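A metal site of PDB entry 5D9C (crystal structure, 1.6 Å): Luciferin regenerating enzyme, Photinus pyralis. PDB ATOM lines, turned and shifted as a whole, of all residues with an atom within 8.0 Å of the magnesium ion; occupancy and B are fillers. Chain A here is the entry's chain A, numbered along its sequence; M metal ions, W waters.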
ATOM      1  N   VAL A  19     -33.684 -23.063  25.884  1.00  0.00           N
ATOM      2  CA  VAL A  19     -32.458 -22.287  25.849  1.00  0.00           C
ATOM      3  C   VAL A  19     -32.803 -20.874  25.295  1.00  0.00           C
ATOM      4  O   VAL A  19     -32.647 -20.604  24.109  1.00  0.00           O
ATOM      5  CB  VAL A  19     -31.337 -22.941  25.003  1.00  0.00           C
ATOM      6  CG1 VAL A  19     -30.030 -22.120  25.097  1.00  0.00           C
ATOM      7  CG2 VAL A  19     -30.996 -24.423  25.460  1.00  0.00           C
ATOM      8  N   GLY A  20     -33.245 -19.992  26.189  1.00  0.00           N
ATOM      9  CA  GLY A  20     -33.409 -18.569  25.866  1.00  0.00           C
ATOM     10  C   GLY A  20     -32.031 -17.998  25.528  1.00  0.00           C
ATOM     11  O   GLY A  20     -31.036 -18.323  26.185  1.00  0.00           O
ATOM     12  N   GLU A  21     -31.955 -17.184  24.466  1.00  0.00           N
ATOM     13  CA  GLU A  21     -30.656 -16.739  23.959  1.00  0.00           C
ATOM     14  C   GLU A  21     -30.813 -15.497  23.093  1.00  0.00           C
ATOM     15  O   GLU A  21     -31.915 -15.082  22.800  1.00  0.00           O
ATOM     16  CB  GLU A  21     -29.972 -17.856  23.151  1.00  0.00           C
ATOM     17  CG  GLU A  21     -28.857 -18.615  23.913  1.00  0.00           C
ATOM     18  CD  GLU A  21     -27.579 -17.820  24.048  1.00  0.00           C
ATOM     19  OE1 GLU A  21     -26.552 -18.424  24.464  1.00  0.00           O
ATOM     20  OE2 GLU A  21     -27.591 -16.598  23.744  1.00  0.00           O
ATOM     21  N   GLY A  22     -29.690 -14.902  22.709  1.00  0.00           N
ATOM     22  CA  GLY A  22     -29.643 -13.844  21.709  1.00  0.00           C
ATOM     23  C   GLY A  22     -30.541 -12.635  21.940  1.00  0.00           C
ATOM     24  O   GLY A  22     -31.200 -12.184  20.993  1.00  0.00           O
ATOM     25  N   PRO A  23     -30.568 -12.078  23.158  1.00  0.00           N
ATOM     26  CA  PRO A  23     -31.443 -10.926  23.388  1.00  0.00           C
ATOM     27  C   PRO A  23     -30.964  -9.708  22.555  1.00  0.00           C
ATOM     28  O   PRO A  23     -29.741  -9.479  22.438  1.00  0.00           O
ATOM     29  CB  PRO A  23     -31.314 -10.679  24.905  1.00  0.00           C
ATOM     30  CG  PRO A  23     -29.950 -11.159  25.236  1.00  0.00           C
ATOM     31  CD  PRO A  23     -29.851 -12.438  24.395  1.00  0.00           C
ATOM     32  N   THR A  37     -32.944 -21.459  21.340  1.00  0.00           N
ATOM     33  CA  THR A  37     -32.031 -22.083  20.381  1.00  0.00           C
ATOM     34  C   THR A  37     -32.245 -23.585  20.225  1.00  0.00           C
ATOM     35  O   THR A  37     -31.580 -24.209  19.405  1.00  0.00           O
ATOM     36  CB  THR A  37     -30.524 -21.831  20.717  1.00  0.00           C
ATOM     37  OG1 THR A  37     -30.139 -22.359  22.009  1.00  0.00           O
ATOM     38  CG2 THR A  37     -30.211 -20.387  20.676  1.00  0.00           C
ATOM     39  N   SER A  62     -30.438 -19.068  16.296  1.00  0.00           N
ATOM     40  CA  SER A  62     -29.556 -18.620  17.343  1.00  0.00           C
ATOM     41  C   SER A  62     -29.448 -17.102  17.490  1.00  0.00           C
ATOM     42  O   SER A  62     -28.913 -16.642  18.477  1.00  0.00           O
ATOM     43  CB  SER A  62     -28.152 -19.203  17.143  1.00  0.00           C
ATOM     44  OG  SER A  62     -27.502 -18.734  15.953  1.00  0.00           O
ATOM     45  N   ASN A 113     -24.184 -20.290  16.023  1.00  0.00           N
ATOM     46  CA  ASN A 113     -24.556 -19.957  17.388  1.00  0.00           C
ATOM     47  C   ASN A 113     -24.601 -18.441  17.519  1.00  0.00           C
ATOM     48  O   ASN A 113     -25.314 -17.769  16.753  1.00  0.00           O
ATOM     49  CB  ASN A 113     -23.609 -20.631  18.406  1.00  0.00           C
ATOM     50  CG  ASN A 113     -24.200 -20.645  19.808  1.00  0.00           C
ATOM     51  OD1 ASN A 113     -25.438 -20.609  19.959  1.00  0.00           O
ATOM     52  ND2 ASN A 113     -23.354 -20.607  20.834  1.00  0.00           N
ATOM     53  N   ASP A 114     -23.835 -17.859  18.434  1.00  0.00           N
ATOM     54  CA  ASP A 114     -24.104 -16.464  18.768  1.00  0.00           C
ATOM     55  C   ASP A 114     -23.715 -15.523  17.623  1.00  0.00           C
ATOM     56  O   ASP A 114     -22.788 -15.795  16.859  1.00  0.00           O
ATOM     57  CB  ASP A 114     -23.395 -16.060  20.070  1.00  0.00           C
ATOM     58  CG  ASP A 114     -24.112 -14.910  20.811  1.00  0.00           C
ATOM     59  OD1 ASP A 114     -25.151 -14.384  20.328  1.00  0.00           O
ATOM     60  OD2 ASP A 114     -23.621 -14.516  21.889  1.00  0.00           O
ATOM     61  N   GLY A 115     -24.436 -14.412  17.494  1.00  0.00           N
ATOM     62  CA  GLY A 115     -24.202 -13.493  16.418  1.00  0.00           C
ATOM     63  C   GLY A 115     -24.625 -12.094  16.853  1.00  0.00           C
ATOM     64  O   GLY A 115     -25.537 -11.939  17.667  1.00  0.00           O
ATOM     65  N   MET A 128     -20.484 -23.962  15.434  1.00  0.00           N
ATOM     66  CA  MET A 128     -20.081 -24.980  16.382  1.00  0.00           C
ATOM     67  C   MET A 128     -20.706 -26.309  15.958  1.00  0.00           C
ATOM     68  O   MET A 128     -21.681 -26.333  15.193  1.00  0.00           O
ATOM     69  CB  MET A 128     -20.527 -24.624  17.794  1.00  0.00           C
ATOM     70  CG  MET A 128     -22.058 -24.359  17.851  1.00  0.00           C
ATOM     71  SD  MET A 128     -22.661 -23.939  19.490  1.00  0.00           S
ATOM     72  CE  MET A 128     -22.208 -25.351  20.473  1.00  0.00           C
ATOM     73  N   ILE A 161     -17.278 -23.619  21.140  1.00  0.00           N
ATOM     74  CA  ILE A 161     -18.633 -23.089  21.296  1.00  0.00           C
ATOM     75  C   ILE A 161     -18.621 -21.588  21.030  1.00  0.00           C
ATOM     76  O   ILE A 161     -18.288 -20.797  21.903  1.00  0.00           O
ATOM     77  CB  ILE A 161     -19.218 -23.356  22.702  1.00  0.00           C
ATOM     78  CG1 ILE A 161     -19.102 -24.873  23.007  1.00  0.00           C
ATOM     79  CG2 ILE A 161     -20.679 -22.795  22.805  1.00  0.00           C
ATOM     80  CD1 ILE A 161     -20.170 -25.420  23.970  1.00  0.00           C
ATOM     81  N   ALA A 162     -18.972 -21.232  19.796  1.00  0.00           N
ATOM     82  CA  ALA A 162     -18.935 -19.857  19.326  1.00  0.00           C
ATOM     83  C   ALA A 162     -19.935 -18.998  20.121  1.00  0.00           C
ATOM     84  O   ALA A 162     -21.170 -19.151  19.985  1.00  0.00           O
ATOM     85  CB  ALA A 162     -19.249 -19.820  17.852  1.00  0.00           C
ATOM     86  N   ASN A 163     -19.433 -18.111  20.963  1.00  0.00           N
ATOM     87  CA  ASN A 163     -20.401 -17.406  21.803  1.00  0.00           C
ATOM     88  C   ASN A 163     -20.201 -15.879  21.793  1.00  0.00           C
ATOM     89  O   ASN A 163     -20.017 -15.319  20.711  1.00  0.00           O
ATOM     90  CB  ASN A 163     -20.387 -18.002  23.209  1.00  0.00           C
ATOM     91  CG  ASN A 163     -21.707 -18.683  23.539  1.00  0.00           C
ATOM     92  OD1 ASN A 163     -22.769 -18.193  23.154  1.00  0.00           O
ATOM     93  ND2 ASN A 163     -21.643 -19.855  24.218  1.00  0.00           N
ATOM     94  N   GLY A 164     -20.312 -15.230  22.957  1.00  0.00           N
ATOM     95  CA  GLY A 164     -20.492 -13.775  23.056  1.00  0.00           C
ATOM     96  C   GLY A 164     -19.475 -12.875  22.371  1.00  0.00           C
ATOM     97  O   GLY A 164     -18.287 -13.176  22.353  1.00  0.00           O
ATOM     98  N   ILE A 177     -15.844 -14.729  22.972  1.00  0.00           N
ATOM     99  CA  ILE A 177     -15.931 -15.878  23.871  1.00  0.00           C
ATOM    100  C   ILE A 177     -16.097 -17.172  23.110  1.00  0.00           C
ATOM    101  O   ILE A 177     -17.061 -17.383  22.361  1.00  0.00           O
ATOM    102  CB  ILE A 177     -17.111 -15.704  24.859  1.00  0.00           C
ATOM    103  CG1 ILE A 177     -16.798 -14.563  25.840  1.00  0.00           C
ATOM    104  CG2 ILE A 177     -17.338 -17.002  25.652  1.00  0.00           C
ATOM    105  CD1 ILE A 177     -18.023 -14.016  26.561  1.00  0.00           C
ATOM    106  N   SER A 179     -16.750 -20.607  24.592  1.00  0.00           N
ATOM    107  CA  SER A 179     -17.104 -21.072  25.929  1.00  0.00           C
ATOM    108  C   SER A 179     -16.184 -22.215  26.403  1.00  0.00           C
ATOM    109  O   SER A 179     -15.903 -22.356  27.598  1.00  0.00           O
ATOM    110  CB  SER A 179     -18.582 -21.524  25.991  1.00  0.00           C
ATOM    111  OG  SER A 179     -19.444 -20.403  25.743  1.00  0.00           O
ATOM    112  N   PRO A 214     -18.243 -18.885  30.348  1.00  0.00           N
ATOM    113  CA  PRO A 214     -18.716 -17.624  29.778  1.00  0.00           C
ATOM    114  C   PRO A 214     -19.593 -17.937  28.549  1.00  0.00           C
ATOM    115  O   PRO A 214     -19.330 -18.912  27.802  1.00  0.00           O
ATOM    116  CB  PRO A 214     -17.416 -16.872  29.397  1.00  0.00           C
ATOM    117  CG  PRO A 214     -16.420 -17.981  29.107  1.00  0.00           C
ATOM    118  CD  PRO A 214     -16.804 -19.137  30.073  1.00  0.00           C
ATOM    119  N   ASP A 215     -20.660 -17.165  28.364  1.00  0.00           N
ATOM    120  CA  ASP A 215     -21.627 -17.482  27.315  1.00  0.00           C
ATOM    121  C   ASP A 215     -21.804 -16.196  26.516  1.00  0.00           C
ATOM    122  O   ASP A 215     -20.915 -15.842  25.742  1.00  0.00           O
ATOM    123  CB  ASP A 215     -22.940 -18.037  27.914  1.00  0.00           C
ATOM    124  CG  ASP A 215     -23.844 -18.740  26.860  1.00  0.00           C
ATOM    125  OD1 ASP A 215     -23.792 -18.333  25.686  1.00  0.00           O
ATOM    126  OD2 ASP A 215     -24.617 -19.699  27.212  1.00  0.00           O
ATOM    127  N   GLY A 216     -22.913 -15.459  26.711  1.00  0.00           N
ATOM    128  CA  GLY A 216     -23.121 -14.190  26.008  1.00  0.00           C
ATOM    129  C   GLY A 216     -22.463 -13.019  26.747  1.00  0.00           C
ATOM    130  O   GLY A 216     -22.165 -13.144  27.937  1.00  0.00           O
ATOM    131  N   GLN A 217     -22.257 -11.894  26.066  1.00  0.00           N
ATOM    132  CA  GLN A 217     -21.684 -10.717  26.751  1.00  0.00           C
ATOM    133  C   GLN A 217     -22.112  -9.454  26.090  1.00  0.00           C
ATOM    134  O   GLN A 217     -22.564  -9.440  24.938  1.00  0.00           O
ATOM    135  CB  GLN A 217     -20.142 -10.806  26.782  1.00  0.00           C
ATOM    136  CG  GLN A 217     -19.464 -10.599  25.402  1.00  0.00           C
ATOM    137  CD  GLN A 217     -17.939 -10.642  25.491  1.00  0.00           C
ATOM    138  OE1 GLN A 217     -17.359 -10.278  26.518  1.00  0.00           O
ATOM    139  NE2 GLN A 217     -17.305 -11.139  24.444  1.00  0.00           N
ATOM    140  N   ALA A 228     -22.449 -13.235  30.842  1.00  0.00           N
ATOM    141  CA  ALA A 228     -23.327 -14.271  31.368  1.00  0.00           C
ATOM    142  C   ALA A 228     -22.520 -15.524  31.714  1.00  0.00           C
ATOM    143  O   ALA A 228     -21.701 -15.945  30.910  1.00  0.00           O
ATOM    144  CB  ALA A 228     -24.398 -14.604  30.311  1.00  0.00           C
ATOM    145  N   PHE A 230     -22.862 -19.337  32.334  1.00  0.00           N
ATOM    146  CA  PHE A 230     -23.672 -20.538  32.201  1.00  0.00           C
ATOM    147  C   PHE A 230     -23.165 -21.584  33.233  1.00  0.00           C
ATOM    148  O   PHE A 230     -21.970 -21.919  33.261  1.00  0.00           O
ATOM    149  CB  PHE A 230     -23.562 -21.056  30.757  1.00  0.00           C
ATOM    150  CG  PHE A 230     -24.501 -22.210  30.434  1.00  0.00           C
ATOM    151  CD1 PHE A 230     -25.794 -21.963  29.950  1.00  0.00           C
ATOM    152  CD2 PHE A 230     -24.093 -23.515  30.625  1.00  0.00           C
ATOM    153  CE1 PHE A 230     -26.651 -23.045  29.637  1.00  0.00           C
ATOM    154  CE2 PHE A 230     -24.944 -24.585  30.314  1.00  0.00           C
ATOM    155  CZ  PHE A 230     -26.222 -24.343  29.826  1.00  0.00           C
ATOM    156  N   VAL A 257     -27.379 -19.102  33.204  1.00  0.00           N
ATOM    157  CA  VAL A 257     -27.476 -17.762  32.586  1.00  0.00           C
ATOM    158  C   VAL A 257     -26.851 -17.819  31.199  1.00  0.00           C
ATOM    159  O   VAL A 257     -25.761 -18.331  31.058  1.00  0.00           O
ATOM    160  CB  VAL A 257     -26.737 -16.704  33.465  1.00  0.00           C
ATOM    161  CG1 VAL A 257     -26.883 -15.318  32.838  1.00  0.00           C
ATOM    162  CG2 VAL A 257     -27.318 -16.711  34.891  1.00  0.00           C
ATOM    163  N   THR A 258     -27.521 -17.319  30.172  1.00  0.00           N
ATOM    164  CA  THR A 258     -26.988 -17.489  28.814  1.00  0.00           C
ATOM    165  C   THR A 258     -26.504 -16.191  28.154  1.00  0.00           C
ATOM    166  O   THR A 258     -25.508 -16.193  27.468  1.00  0.00           O
ATOM    167  CB  THR A 258     -28.015 -18.154  27.863  1.00  0.00           C
ATOM    168  OG1 THR A 258     -29.215 -17.379  27.872  1.00  0.00           O
ATOM    169  CG2 THR A 258     -28.307 -19.631  28.299  1.00  0.00           C
ATOM    170  N   SER A 259     -27.224 -15.103  28.315  1.00  0.00           N
ATOM    171  CA  SER A 259     -26.801 -13.861  27.632  1.00  0.00           C
ATOM    172  C   SER A 259     -27.437 -12.626  28.254  1.00  0.00           C
ATOM    173  O   SER A 259     -28.231 -12.725  29.169  1.00  0.00           O
ATOM    174  CB  SER A 259     -27.132 -13.930  26.131  1.00  0.00           C
ATOM    175  OG  SER A 259     -26.407 -12.957  25.385  1.00  0.00           O
ATOM    176  N   THR A 273     -31.166 -13.542  29.709  1.00  0.00           N
ATOM    177  CA  THR A 273     -31.823 -14.793  29.379  1.00  0.00           C
ATOM    178  C   THR A 273     -31.154 -15.986  30.111  1.00  0.00           C
ATOM    179  O   THR A 273     -30.005 -15.897  30.535  1.00  0.00           O
ATOM    180  CB  THR A 273     -31.748 -15.067  27.865  1.00  0.00           C
ATOM    181  OG1 THR A 273     -30.407 -14.916  27.430  1.00  0.00           O
ATOM    182  CG2 THR A 273     -32.582 -14.053  27.092  1.00  0.00           C
HETATM  183 MG    MG M   1     -24.653 -18.220  23.891  1.00  0.00          MG
HETATM  184  O   HOH W   1     -24.687 -20.395  23.511  1.00  0.00           O
HETATM  185  O   HOH W   2     -25.489 -18.217  21.699  1.00  0.00           O
HETATM  186  O   HOH W   3     -24.895 -16.160  23.887  1.00  0.00           O
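The magnesium ion is bound by OE1 of Glu 21 (2.0 Å), OD1 of Asp 215 (2.0 Å), OD1 of Asn 163 (2.0 Å), water W3 (2.1 Å), water W1 (2.2 Å) and water W2 (2.3 Å).
The backbone NH of Gly 164 sits at hydrogen-bond distance from the backbone carbonyl oxygen of Asp 215 (2.9 Å). N of Asp 215 sits at hydrogen-bond distance from O of Ala 228 (3.0 Å). OD1 of Asn 163 lies close to ND2 of Asn 113 (3.4 Å). The side-chain hydroxyl of Ser 179 is in hydrogen-bond range of the side-chain amide nitrogen of Asn 163 (2.7 Å). The backbone NH (N) of Asn 163 sits at hydrogen-bond distance from the backbone carbonyl oxygen (O) of Ile 177, at 2.8 Å.
Water W2 bridges OD1 of Asn 113 and OE2 of Glu 21. Water W1 bridges ND2 of Asn 113 (3.0 Å) and ND2 of Asn 163 (3.2 Å). Water W3 bridges the side-chain carboxylate of Glu 21 (2.7 Å) and the side-chain carboxylate of Asp 114 (2.9 Å).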
